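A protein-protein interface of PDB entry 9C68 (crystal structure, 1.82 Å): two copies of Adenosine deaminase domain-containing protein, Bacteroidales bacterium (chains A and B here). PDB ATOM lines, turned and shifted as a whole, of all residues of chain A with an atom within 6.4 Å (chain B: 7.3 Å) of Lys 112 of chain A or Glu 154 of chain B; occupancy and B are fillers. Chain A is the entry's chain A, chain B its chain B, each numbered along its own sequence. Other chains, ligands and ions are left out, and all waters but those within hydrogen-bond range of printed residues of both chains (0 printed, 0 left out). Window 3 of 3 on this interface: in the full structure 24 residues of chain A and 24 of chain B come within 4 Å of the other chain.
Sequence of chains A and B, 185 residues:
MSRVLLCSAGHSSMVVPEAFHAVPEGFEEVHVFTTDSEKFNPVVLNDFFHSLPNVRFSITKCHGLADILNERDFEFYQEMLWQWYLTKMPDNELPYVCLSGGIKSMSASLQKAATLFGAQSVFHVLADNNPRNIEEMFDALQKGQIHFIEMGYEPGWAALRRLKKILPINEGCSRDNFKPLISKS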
ATOM      1  N   GLN A  78       0.308 -10.555   5.548  1.00  0.00           N
ATOM      2  CA  GLN A  78       1.374 -11.550   5.400  1.00  0.00           C
ATOM      3  C   GLN A  78       0.831 -12.950   5.164  1.00  0.00           C
ATOM      4  O   GLN A  78       1.341 -13.689   4.313  1.00  0.00           O
ATOM      5  CB  GLN A  78       2.255 -11.541   6.646  1.00  0.00           C
ATOM      6  CG  GLN A  78       3.498 -12.383   6.507  1.00  0.00           C
ATOM      7  CD  GLN A  78       4.692 -11.761   7.201  1.00  0.00           C
ATOM      8  OE1 GLN A  78       4.904 -11.970   8.403  1.00  0.00           O
ATOM      9  NE2 GLN A  78       5.472 -10.962   6.452  1.00  0.00           N
ATOM     10  N   TRP A  82       1.577 -15.037   1.792  1.00  0.00           N
ATOM     11  CA  TRP A  82       2.304 -16.309   1.770  1.00  0.00           C
ATOM     12  C   TRP A  82       1.435 -17.435   1.238  1.00  0.00           C
ATOM     13  O   TRP A  82       1.929 -18.321   0.527  1.00  0.00           O
ATOM     14  CB  TRP A  82       2.825 -16.644   3.163  1.00  0.00           C
ATOM     15  CG  TRP A  82       3.851 -15.687   3.641  1.00  0.00           C
ATOM     16  CD1 TRP A  82       4.290 -14.569   3.001  1.00  0.00           C
ATOM     17  CD2 TRP A  82       4.586 -15.771   4.853  1.00  0.00           C
ATOM     18  NE1 TRP A  82       5.251 -13.929   3.758  1.00  0.00           N
ATOM     19  CE2 TRP A  82       5.452 -14.658   4.897  1.00  0.00           C
ATOM     20  CE3 TRP A  82       4.586 -16.672   5.926  1.00  0.00           C
ATOM     21  CZ2 TRP A  82       6.312 -14.426   5.966  1.00  0.00           C
ATOM     22  CZ3 TRP A  82       5.440 -16.442   6.984  1.00  0.00           C
ATOM     23  CH2 TRP A  82       6.289 -15.323   7.000  1.00  0.00           C
ATOM     24  N   SER A 107       6.289  -4.663   0.286  1.00  0.00           N
ATOM     25  CA  SER A 107       7.503  -5.039  -0.442  1.00  0.00           C
ATOM     26  C   SER A 107       8.399  -5.926   0.424  1.00  0.00           C
ATOM     27  O   SER A 107       8.850  -6.998  -0.011  1.00  0.00           O
ATOM     28  CB  SER A 107       8.211  -3.758  -0.902  1.00  0.00           C
ATOM     29  OG  SER A 107       9.517  -4.031  -1.338  1.00  0.00           O
ATOM     30  N   ALA A 108       8.623  -5.513   1.674  1.00  0.00           N
ATOM     31  CA  ALA A 108       9.423  -6.288   2.623  1.00  0.00           C
ATOM     32  C   ALA A 108       8.862  -7.693   2.838  1.00  0.00           C
ATOM     33  O   ALA A 108       9.625  -8.659   2.965  1.00  0.00           O
ATOM     34  CB  ALA A 108       9.499  -5.546   3.960  1.00  0.00           C
ATOM     35  N   SER A 109       7.535  -7.823   2.907  1.00  0.00           N
ATOM     36  CA  SER A 109       6.915  -9.123   3.132  1.00  0.00           C
ATOM     37  C   SER A 109       7.090 -10.048   1.927  1.00  0.00           C
ATOM     38  O   SER A 109       7.262 -11.263   2.085  1.00  0.00           O
ATOM     39  CB  SER A 109       5.430  -8.939   3.452  1.00  0.00           C
ATOM     40  OG  SER A 109       4.800 -10.164   3.783  1.00  0.00           O
ATOM     41  N   LEU A 110       7.004  -9.507   0.704  1.00  0.00           N
ATOM     42  CA  LEU A 110       7.283 -10.339  -0.465  1.00  0.00           C
ATOM     43  C   LEU A 110       8.747 -10.770  -0.516  1.00  0.00           C
ATOM     44  O   LEU A 110       9.049 -11.912  -0.886  1.00  0.00           O
ATOM     45  CB  LEU A 110       6.894  -9.603  -1.757  1.00  0.00           C
ATOM     46  CG  LEU A 110       6.935 -10.417  -3.069  1.00  0.00           C
ATOM     47  CD1 LEU A 110       6.213 -11.778  -3.030  1.00  0.00           C
ATOM     48  CD2 LEU A 110       6.297  -9.539  -4.160  1.00  0.00           C
ATOM     49  N   GLN A 111       9.673  -9.873  -0.192  1.00  0.00           N
ATOM     50  CA  GLN A 111      11.062 -10.293  -0.056  1.00  0.00           C
ATOM     51  C   GLN A 111      11.177 -11.480   0.897  1.00  0.00           C
ATOM     52  O   GLN A 111      11.848 -12.480   0.595  1.00  0.00           O
ATOM     53  CB  GLN A 111      11.926  -9.132   0.434  1.00  0.00           C
ATOM     54  CG  GLN A 111      13.316  -9.534   0.842  1.00  0.00           C
ATOM     55  CD  GLN A 111      14.202  -9.805  -0.358  1.00  0.00           C
ATOM     56  OE1 GLN A 111      14.574  -8.889  -1.070  1.00  0.00           O
ATOM     57  NE2 GLN A 111      14.474 -11.073  -0.629  1.00  0.00           N
ATOM     58  N   LYS A 112      10.496 -11.398   2.045  1.00  0.00           N
ATOM     59  CA  LYS A 112      10.582 -12.486   3.021  1.00  0.00           C
ATOM     60  C   LYS A 112       9.975 -13.771   2.473  1.00  0.00           C
ATOM     61  O   LYS A 112      10.504 -14.867   2.704  1.00  0.00           O
ATOM     62  CB  LYS A 112       9.885 -12.061   4.320  1.00  0.00           C
ATOM     63  CG  LYS A 112      10.368 -12.765   5.549  1.00  0.00           C
ATOM     64  CD  LYS A 112       9.616 -12.356   6.828  1.00  0.00           C
ATOM     65  CE  LYS A 112       9.286 -13.580   7.675  1.00  0.00           C
ATOM     66  NZ  LYS A 112       9.193 -13.233   9.136  1.00  0.00           N
ATOM     67  N   ALA A 113       8.860 -13.669   1.747  1.00  0.00           N
ATOM     68  CA  ALA A 113       8.287 -14.861   1.133  1.00  0.00           C
ATOM     69  C   ALA A 113       9.257 -15.484   0.140  1.00  0.00           C
ATOM     70  O   ALA A 113       9.435 -16.708   0.118  1.00  0.00           O
ATOM     71  CB  ALA A 113       6.966 -14.534   0.435  1.00  0.00           C
ATOM     72  N   ALA A 114       9.891 -14.649  -0.699  1.00  0.00           N
ATOM     73  CA  ALA A 114      10.902 -15.146  -1.631  1.00  0.00           C
ATOM     74  C   ALA A 114      12.001 -15.900  -0.896  1.00  0.00           C
ATOM     75  O   ALA A 114      12.420 -16.989  -1.324  1.00  0.00           O
ATOM     76  CB  ALA A 114      11.485 -13.973  -2.432  1.00  0.00           C
ATOM     77  N   THR A 115      12.483 -15.322   0.204  1.00  0.00           N
ATOM     78  CA  THR A 115      13.557 -15.925   0.976  1.00  0.00           C
ATOM     79  C   THR A 115      13.118 -17.276   1.556  1.00  0.00           C
ATOM     80  O   THR A 115      13.904 -18.233   1.568  1.00  0.00           O
ATOM     81  CB  THR A 115      14.008 -14.937   2.070  1.00  0.00           C
ATOM     82  OG1 THR A 115      14.722 -13.823   1.483  1.00  0.00           O
ATOM     83  CG2 THR A 115      14.942 -15.593   3.021  1.00  0.00           C
ATOM     84  N   LEU A 116      11.843 -17.401   1.983  1.00  0.00           N
ATOM     85  CA  LEU A 116      11.353 -18.666   2.553  1.00  0.00           C
ATOM     86  C   LEU A 116      10.972 -19.698   1.497  1.00  0.00           C
ATOM     87  O   LEU A 116      11.268 -20.890   1.661  1.00  0.00           O
ATOM     88  CB  LEU A 116      10.146 -18.458   3.485  1.00  0.00           C
ATOM     89  CG  LEU A 116      10.164 -17.476   4.667  1.00  0.00           C
ATOM     90  CD1 LEU A 116       8.772 -17.021   5.025  1.00  0.00           C
ATOM     91  CD2 LEU A 116      10.861 -18.084   5.891  1.00  0.00           C
ATOM     92  N   PHE A 117      10.260 -19.295   0.440  1.00  0.00           N
ATOM     93  CA  PHE A 117       9.758 -20.267  -0.511  1.00  0.00           C
ATOM     94  C   PHE A 117      10.639 -20.394  -1.750  1.00  0.00           C
ATOM     95  O   PHE A 117      10.458 -21.337  -2.517  1.00  0.00           O
ATOM     96  CB  PHE A 117       8.315 -19.929  -0.936  1.00  0.00           C
ATOM     97  CG  PHE A 117       7.360 -19.774   0.226  1.00  0.00           C
ATOM     98  CD1 PHE A 117       7.265 -20.757   1.188  1.00  0.00           C
ATOM     99  CD2 PHE A 117       6.627 -18.598   0.391  1.00  0.00           C
ATOM    100  CE1 PHE A 117       6.398 -20.616   2.276  1.00  0.00           C
ATOM    101  CE2 PHE A 117       5.764 -18.439   1.476  1.00  0.00           C
ATOM    102  CZ  PHE A 117       5.649 -19.459   2.418  1.00  0.00           C
ATOM    103  N   TYR B  85      24.939  -3.779   9.803  1.00  0.00           N
ATOM    104  CA  TYR B  85      24.041  -4.481  10.715  1.00  0.00           C
ATOM    105  C   TYR B  85      24.818  -5.286  11.763  1.00  0.00           C
ATOM    106  O   TYR B  85      24.659  -5.094  12.977  1.00  0.00           O
ATOM    107  CB  TYR B  85      23.133  -5.378   9.887  1.00  0.00           C
ATOM    108  CG  TYR B  85      21.903  -5.868  10.599  1.00  0.00           C
ATOM    109  CD1 TYR B  85      21.989  -6.816  11.619  1.00  0.00           C
ATOM    110  CD2 TYR B  85      20.647  -5.375  10.267  1.00  0.00           C
ATOM    111  CE1 TYR B  85      20.870  -7.274  12.268  1.00  0.00           C
ATOM    112  CE2 TYR B  85      19.503  -5.831  10.913  1.00  0.00           C
ATOM    113  CZ  TYR B  85      19.627  -6.769  11.922  1.00  0.00           C
ATOM    114  OH  TYR B  85      18.501  -7.221  12.571  1.00  0.00           O
ATOM    115  N   LEU B  94      19.051  -8.823  20.666  1.00  0.00           N
ATOM    116  CA  LEU B  94      18.726  -8.545  19.269  1.00  0.00           C
ATOM    117  C   LEU B  94      18.350  -7.069  19.091  1.00  0.00           C
ATOM    118  O   LEU B  94      17.780  -6.450  19.996  1.00  0.00           O
ATOM    119  CB  LEU B  94      17.580  -9.439  18.810  1.00  0.00           C
ATOM    120  CG  LEU B  94      17.970 -10.925  18.804  1.00  0.00           C
ATOM    121  CD1 LEU B  94      16.896 -11.816  18.227  1.00  0.00           C
ATOM    122  CD2 LEU B  94      19.294 -11.135  18.075  1.00  0.00           C
ATOM    123  N   PRO B  95      18.672  -6.472  17.946  1.00  0.00           N
ATOM    124  CA  PRO B  95      18.350  -5.055  17.720  1.00  0.00           C
ATOM    125  C   PRO B  95      16.887  -4.859  17.336  1.00  0.00           C
ATOM    126  O   PRO B  95      16.175  -5.808  17.019  1.00  0.00           O
ATOM    127  CB  PRO B  95      19.272  -4.690  16.553  1.00  0.00           C
ATOM    128  CG  PRO B  95      19.307  -5.946  15.738  1.00  0.00           C
ATOM    129  CD  PRO B  95      19.324  -7.081  16.768  1.00  0.00           C
ATOM    130  N   ALA B 108      13.775  -3.825   1.548  1.00  0.00           N
ATOM    131  CA  ALA B 108      13.785  -5.282   1.440  1.00  0.00           C
ATOM    132  C   ALA B 108      15.121  -5.866   1.887  1.00  0.00           C
ATOM    133  O   ALA B 108      15.155  -6.937   2.495  1.00  0.00           O
ATOM    134  CB  ALA B 108      13.446  -5.723   0.011  1.00  0.00           C
ATOM    135  N   GLN B 111      15.083  -5.878   5.662  1.00  0.00           N
ATOM    136  CA  GLN B 111      14.208  -6.962   6.106  1.00  0.00           C
ATOM    137  C   GLN B 111      14.930  -8.301   6.047  1.00  0.00           C
ATOM    138  O   GLN B 111      14.871  -9.106   6.985  1.00  0.00           O
ATOM    139  CB  GLN B 111      12.954  -7.021   5.229  1.00  0.00           C
ATOM    140  CG  GLN B 111      12.089  -8.267   5.419  1.00  0.00           C
ATOM    141  CD  GLN B 111      11.356  -8.274   6.771  1.00  0.00           C
ATOM    142  OE1 GLN B 111      10.335  -7.602   6.944  1.00  0.00           O
ATOM    143  NE2 GLN B 111      11.893  -9.030   7.741  1.00  0.00           N
ATOM    144  N   LYS B 112      15.611  -8.558   4.931  1.00  0.00           N
ATOM    145  CA  LYS B 112      16.324  -9.815   4.777  1.00  0.00           C
ATOM    146  C   LYS B 112      17.465  -9.920   5.786  1.00  0.00           C
ATOM    147  O   LYS B 112      17.687 -10.999   6.352  1.00  0.00           O
ATOM    148  CB  LYS B 112      16.810  -9.944   3.319  1.00  0.00           C
ATOM    149  CG  LYS B 112      17.901 -10.959   3.080  1.00  0.00           C
ATOM    150  CD  LYS B 112      17.736 -11.596   1.692  1.00  0.00           C
ATOM    151  CE  LYS B 112      18.497 -12.934   1.539  1.00  0.00           C
ATOM    152  NZ  LYS B 112      19.124 -13.023   0.147  1.00  0.00           N
ATOM    153  N   ALA B 113      18.177  -8.809   6.064  1.00  0.00           N
ATOM    154  CA  ALA B 113      19.242  -8.858   7.068  1.00  0.00           C
ATOM    155  C   ALA B 113      18.680  -9.196   8.445  1.00  0.00           C
ATOM    156  O   ALA B 113      19.255  -9.993   9.198  1.00  0.00           O
ATOM    157  CB  ALA B 113      19.991  -7.523   7.121  1.00  0.00           C
ATOM    158  N   ALA B 114      17.545  -8.598   8.779  1.00  0.00           N
ATOM    159  CA  ALA B 114      16.867  -8.899  10.031  1.00  0.00           C
ATOM    160  C   ALA B 114      16.448 -10.372  10.104  1.00  0.00           C
ATOM    161  O   ALA B 114      16.551 -11.014  11.163  1.00  0.00           O
ATOM    162  CB  ALA B 114      15.678  -7.948  10.153  1.00  0.00           C
ATOM    163  N   THR B 115      16.014 -10.946   8.982  1.00  0.00           N
ATOM    164  CA  THR B 115      15.667 -12.356   9.006  1.00  0.00           C
ATOM    165  C   THR B 115      16.891 -13.239   9.201  1.00  0.00           C
ATOM    166  O   THR B 115      16.773 -14.345   9.726  1.00  0.00           O
ATOM    167  CB  THR B 115      14.954 -12.767   7.732  1.00  0.00           C
ATOM    168  OG1 THR B 115      15.879 -12.689   6.639  1.00  0.00           O
ATOM    169  CG2 THR B 115      13.736 -11.887   7.495  1.00  0.00           C
ATOM    170  N   LEU B 116      18.064 -12.777   8.787  1.00  0.00           N
ATOM    171  CA  LEU B 116      19.251 -13.617   8.877  1.00  0.00           C
ATOM    172  C   LEU B 116      19.935 -13.473  10.235  1.00  0.00           C
ATOM    173  O   LEU B 116      20.247 -14.474  10.891  1.00  0.00           O
ATOM    174  CB  LEU B 116      20.220 -13.254   7.740  1.00  0.00           C
ATOM    175  CG  LEU B 116      19.804 -13.708   6.350  1.00  0.00           C
ATOM    176  CD1 LEU B 116      20.938 -13.400   5.372  1.00  0.00           C
ATOM    177  CD2 LEU B 116      19.470 -15.174   6.345  1.00  0.00           C
ATOM    178  N   PHE B 117      20.176 -12.234  10.663  1.00  0.00           N
ATOM    179  CA  PHE B 117      20.942 -11.962  11.862  1.00  0.00           C
ATOM    180  C   PHE B 117      20.075 -11.792  13.103  1.00  0.00           C
ATOM    181  O   PHE B 117      20.610 -11.804  14.215  1.00  0.00           O
ATOM    182  CB  PHE B 117      21.799 -10.707  11.662  1.00  0.00           C
ATOM    183  CG  PHE B 117      22.568 -10.707  10.366  1.00  0.00           C
ATOM    184  CD1 PHE B 117      23.275 -11.836   9.969  1.00  0.00           C
ATOM    185  CD2 PHE B 117      22.559  -9.589   9.526  1.00  0.00           C
ATOM    186  CE1 PHE B 117      23.978 -11.848   8.772  1.00  0.00           C
ATOM    187  CE2 PHE B 117      23.268  -9.590   8.335  1.00  0.00           C
ATOM    188  CZ  PHE B 117      23.975 -10.720   7.959  1.00  0.00           C
ATOM    189  N   GLY B 118      18.763 -11.625  12.948  1.00  0.00           N
ATOM    190  CA  GLY B 118      17.917 -11.473  14.125  1.00  0.00           C
ATOM    191  C   GLY B 118      17.489 -10.061  14.474  1.00  0.00           C
ATOM    192  O   GLY B 118      18.252  -9.094  14.322  1.00  0.00           O
ATOM    193  N   ALA B 119      16.248  -9.916  14.942  1.00  0.00           N
ATOM    194  CA  ALA B 119      15.776  -8.612  15.373  1.00  0.00           C
ATOM    195  C   ALA B 119      14.663  -8.769  16.392  1.00  0.00           C
ATOM    196  O   ALA B 119      13.748  -9.572  16.199  1.00  0.00           O
ATOM    197  CB  ALA B 119      15.258  -7.758  14.208  1.00  0.00           C
ATOM    198  N   GLN B 120      14.742  -7.970  17.460  1.00  0.00           N
ATOM    199  CA  GLN B 120      13.695  -7.993  18.470  1.00  0.00           C
ATOM    200  C   GLN B 120      12.357  -7.600  17.862  1.00  0.00           C
ATOM    201  O   GLN B 120      11.311  -8.181  18.187  1.00  0.00           O
ATOM    202  CB  GLN B 120      14.070  -7.052  19.614  1.00  0.00           C
ATOM    203  CG  GLN B 120      13.141  -7.192  20.805  1.00  0.00           C
ATOM    204  CD  GLN B 120      13.380  -8.506  21.524  1.00  0.00           C
ATOM    205  OE1 GLN B 120      12.442  -9.155  21.978  1.00  0.00           O
ATOM    206  NE2 GLN B 120      14.647  -8.912  21.611  1.00  0.00           N
ATOM    207  N   SER B 121      12.371  -6.616  16.965  1.00  0.00           N
ATOM    208  CA  SER B 121      11.188  -6.270  16.204  1.00  0.00           C
ATOM    209  C   SER B 121      11.646  -5.635  14.899  1.00  0.00           C
ATOM    210  O   SER B 121      12.677  -4.956  14.842  1.00  0.00           O
ATOM    211  CB  SER B 121      10.261  -5.311  16.974  1.00  0.00           C
ATOM    212  OG  SER B 121      10.680  -3.955  16.866  1.00  0.00           O
ATOM    213  N   VAL B 122      10.876  -5.886  13.850  1.00  0.00           N
ATOM    214  CA  VAL B 122      11.009  -5.177  12.587  1.00  0.00           C
ATOM    215  C   VAL B 122       9.745  -4.358  12.426  1.00  0.00           C
ATOM    216  O   VAL B 122       8.645  -4.908  12.521  1.00  0.00           O
ATOM    217  CB  VAL B 122      11.177  -6.160  11.417  1.00  0.00           C
ATOM    218  CG1 VAL B 122      11.310  -5.408  10.081  1.00  0.00           C
ATOM    219  CG2 VAL B 122      12.361  -7.049  11.674  1.00  0.00           C
ATOM    220  N   GLU B 150       4.095  -3.266  13.512  1.00  0.00           N
ATOM    221  CA  GLU B 150       4.967  -4.363  13.905  1.00  0.00           C
ATOM    222  C   GLU B 150       4.797  -5.502  12.916  1.00  0.00           C
ATOM    223  O   GLU B 150       3.699  -6.038  12.747  1.00  0.00           O
ATOM    224  CB  GLU B 150       4.647  -4.829  15.327  1.00  0.00           C
ATOM    225  CG  GLU B 150       5.510  -6.003  15.793  1.00  0.00           C
ATOM    226  CD  GLU B 150       6.977  -5.665  15.748  1.00  0.00           C
ATOM    227  OE1 GLU B 150       7.327  -4.549  16.215  1.00  0.00           O
ATOM    228  OE2 GLU B 150       7.784  -6.508  15.260  1.00  0.00           O
ATOM    229  N   MET B 151       5.886  -5.893  12.272  1.00  0.00           N
ATOM    230  CA  MET B 151       5.818  -6.950  11.278  1.00  0.00           C
ATOM    231  C   MET B 151       6.571  -8.210  11.692  1.00  0.00           C
ATOM    232  O   MET B 151       6.646  -9.152  10.905  1.00  0.00           O
ATOM    233  CB  MET B 151       6.249  -6.408   9.896  1.00  0.00           C
ATOM    234  CG  MET B 151       7.239  -5.275   9.885  1.00  0.00           C
ATOM    235  SD  MET B 151       7.261  -4.171   8.399  1.00  0.00           S
ATOM    236  CE  MET B 151       7.570  -5.396   7.122  1.00  0.00           C
ATOM    237  N   GLY B 152       7.071  -8.282  12.929  1.00  0.00           N
ATOM    238  CA  GLY B 152       7.461  -9.566  13.469  1.00  0.00           C
ATOM    239  C   GLY B 152       8.818  -9.638  14.137  1.00  0.00           C
ATOM    240  O   GLY B 152       9.788  -9.025  13.688  1.00  0.00           O
ATOM    241  N   TYR B 153       8.890 -10.403  15.223  1.00  0.00           N
ATOM    242  CA  TYR B 153      10.168 -10.843  15.767  1.00  0.00           C
ATOM    243  C   TYR B 153      10.888 -11.717  14.747  1.00  0.00           C
ATOM    244  O   TYR B 153      10.261 -12.490  14.023  1.00  0.00           O
ATOM    245  CB  TYR B 153       9.915 -11.635  17.060  1.00  0.00           C
ATOM    246  CG  TYR B 153      11.148 -12.127  17.795  1.00  0.00           C
ATOM    247  CD1 TYR B 153      11.881 -11.272  18.619  1.00  0.00           C
ATOM    248  CD2 TYR B 153      11.577 -13.448  17.673  1.00  0.00           C
ATOM    249  CE1 TYR B 153      13.010 -11.723  19.308  1.00  0.00           C
ATOM    250  CE2 TYR B 153      12.711 -13.908  18.353  1.00  0.00           C
ATOM    251  CZ  TYR B 153      13.422 -13.043  19.163  1.00  0.00           C
ATOM    252  OH  TYR B 153      14.545 -13.495  19.838  1.00  0.00           O
ATOM    253  N   GLU B 154      12.211 -11.593  14.682  1.00  0.00           N
ATOM    254  CA  GLU B 154      13.032 -12.581  13.986  1.00  0.00           C
ATOM    255  C   GLU B 154      14.170 -13.105  14.852  1.00  0.00           C
ATOM    256  O   GLU B 154      15.023 -12.316  15.305  1.00  0.00           O
ATOM    257  CB  GLU B 154      13.564 -12.071  12.649  1.00  0.00           C
ATOM    258  CG  GLU B 154      12.550 -11.290  11.795  1.00  0.00           C
ATOM    259  CD  GLU B 154      11.975 -12.207  10.771  1.00  0.00           C
ATOM    260  OE1 GLU B 154      11.075 -11.806   9.995  1.00  0.00           O
ATOM    261  OE2 GLU B 154      12.432 -13.372  10.759  1.00  0.00           O
ATOM    262  N   PRO B 155      14.233 -14.413  15.070  1.00  0.00           N
ATOM    263  CA  PRO B 155      15.345 -14.983  15.838  1.00  0.00           C
ATOM    264  C   PRO B 155      16.668 -14.870  15.122  1.00  0.00           C
ATOM    265  O   PRO B 155      17.705 -14.703  15.776  1.00  0.00           O
ATOM    266  CB  PRO B 155      14.948 -16.461  16.001  1.00  0.00           C
ATOM    267  CG  PRO B 155      13.631 -16.638  15.267  1.00  0.00           C
ATOM    268  CD  PRO B 155      13.410 -15.444  14.418  1.00  0.00           C
ATOM    269  N   GLY B 156      16.667 -14.971  13.800  1.00  0.00           N
ATOM    270  CA  GLY B 156      17.926 -15.064  13.126  1.00  0.00           C
ATOM    271  C   GLY B 156      18.553 -16.425  13.370  1.00  0.00           C
ATOM    272  O   GLY B 156      17.906 -17.392  13.800  1.00  0.00           O
ATOM    273  N   TRP B 157      19.847 -16.485  13.076  1.00  0.00           N
ATOM    274  CA  TRP B 157      20.614 -17.720  13.154  1.00  0.00           C
ATOM    275  C   TRP B 157      21.901 -17.398  13.873  1.00  0.00           C
ATOM    276  O   TRP B 157      22.620 -16.476  13.463  1.00  0.00           O
ATOM    277  CB  TRP B 157      20.916 -18.289  11.778  1.00  0.00           C
ATOM    278  CG  TRP B 157      19.707 -18.688  11.049  1.00  0.00           C
ATOM    279  CD1 TRP B 157      18.942 -17.894  10.238  1.00  0.00           C
ATOM    280  CD2 TRP B 157      19.092 -19.970  11.061  1.00  0.00           C
ATOM    281  NE1 TRP B 157      17.889 -18.618   9.741  1.00  0.00           N
ATOM    282  CE2 TRP B 157      17.957 -19.895  10.233  1.00  0.00           C
ATOM    283  CE3 TRP B 157      19.389 -21.183  11.690  1.00  0.00           C
ATOM    284  CZ2 TRP B 157      17.124 -20.991  10.014  1.00  0.00           C
ATOM    285  CZ3 TRP B 157      18.563 -22.267  11.468  1.00  0.00           C
ATOM    286  CH2 TRP B 157      17.442 -22.164  10.641  1.00  0.00           C
ATOM    287  N   ARG B 161      24.994 -14.689  13.002  1.00  0.00           N
ATOM    288  CA  ARG B 161      25.506 -13.630  13.864  1.00  0.00           C
ATOM    289  C   ARG B 161      26.998 -13.767  14.088  1.00  0.00           C
ATOM    290  O   ARG B 161      27.683 -12.762  14.346  1.00  0.00           O
ATOM    291  CB  ARG B 161      24.793 -13.632  15.222  1.00  0.00           C
ATOM    292  CG  ARG B 161      23.407 -13.002  15.200  1.00  0.00           C
ATOM    293  CD  ARG B 161      22.810 -12.845  16.600  1.00  0.00           C
ATOM    294  NE  ARG B 161      22.338 -14.121  17.120  1.00  0.00           N
ATOM    295  CZ  ARG B 161      21.178 -14.700  16.827  1.00  0.00           C
ATOM    296  NH1 ARG B 161      20.341 -14.172  15.944  1.00  0.00           N
ATOM    297  NH2 ARG B 161      20.857 -15.851  17.425  1.00  0.00           N
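Among the printed residues, merely in contact across the chains: Ala 108 of chain A with Gln 111 of chain B (3.5 Å), Gln 111 of chain A with Ala 108 of chain B (3.5 Å), Ala 108 of chain A with Met 151 of chain B (3.7 Å), Thr 115 of chain A with Lys 112 of chain B (3.8 Å) and Lys 112 of chain A with Thr 115 of chain B (3.99 Å).
NZ of Lys 112 of chain A lies within salt-bridge range of OE1 of Glu 154 of chain B, at 2.5 Å.
Ala 108 of chain A touches Gln 111 of chain B, and with the chains exchanged Gln 111 of chain A touches Ala 108 of chain B. Lys 112 of chain A touches Thr 115 of chain B, and with the chains exchanged Thr 115 of chain A touches Lys 112 of chain B. 8 positions are printed for both chains.
Ser 107 of chain A touches none of the printed residues of chain B. Of the printed residues of chain B, Lys 112 of chain A touches Thr 115 and Glu 154. Leu 116 of chain A touches none of the printed residues of chain B. Of the printed residues of chain A, Ala 108 of chain B touches Gln 111 (3.5 Å). Printed residues of chain A within 4 Å of Thr 115 of chain B: Lys 112. The nearest printed residue of chain A that does not touch Glu 154 of chain B is Gln 78 of chain A (6.4 Å).
Hydrophobic or aromatic side chains of chain A within 4 Å of the printed part of chain B: Ala 108. Along chain B the printed residues that touch a printed residue of chain A span positions 108 to 154. Among the printed residues, Asp or Glu carboxylates within 4 Å of a Lys or Arg side-chain nitrogen of the other chain: Lys 112 of chain A with Glu 154 of chain B.
The backbone NH (N) of Ala 119 of chain B sits at hydrogen-bond distance from the backbone carbonyl oxygen (O) of Glu 154 of chain B. The backbone carbonyl oxygen (O) of Gln 111 of chain A lies within hydrogen-bond range of the side-chain hydroxyl (OG1) of Thr 115 of chain A (3.3 Å). OG1 of Thr 115 of chain B sits at hydrogen-bond distance from O of Lys 112 of chain B (2.5 Å). The backbone carbonyl oxygen (O) of Val 122 of chain B sits at hydrogen-bond distance from the backbone NH (N) of Met 151 of chain B, at 2.9 Å.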
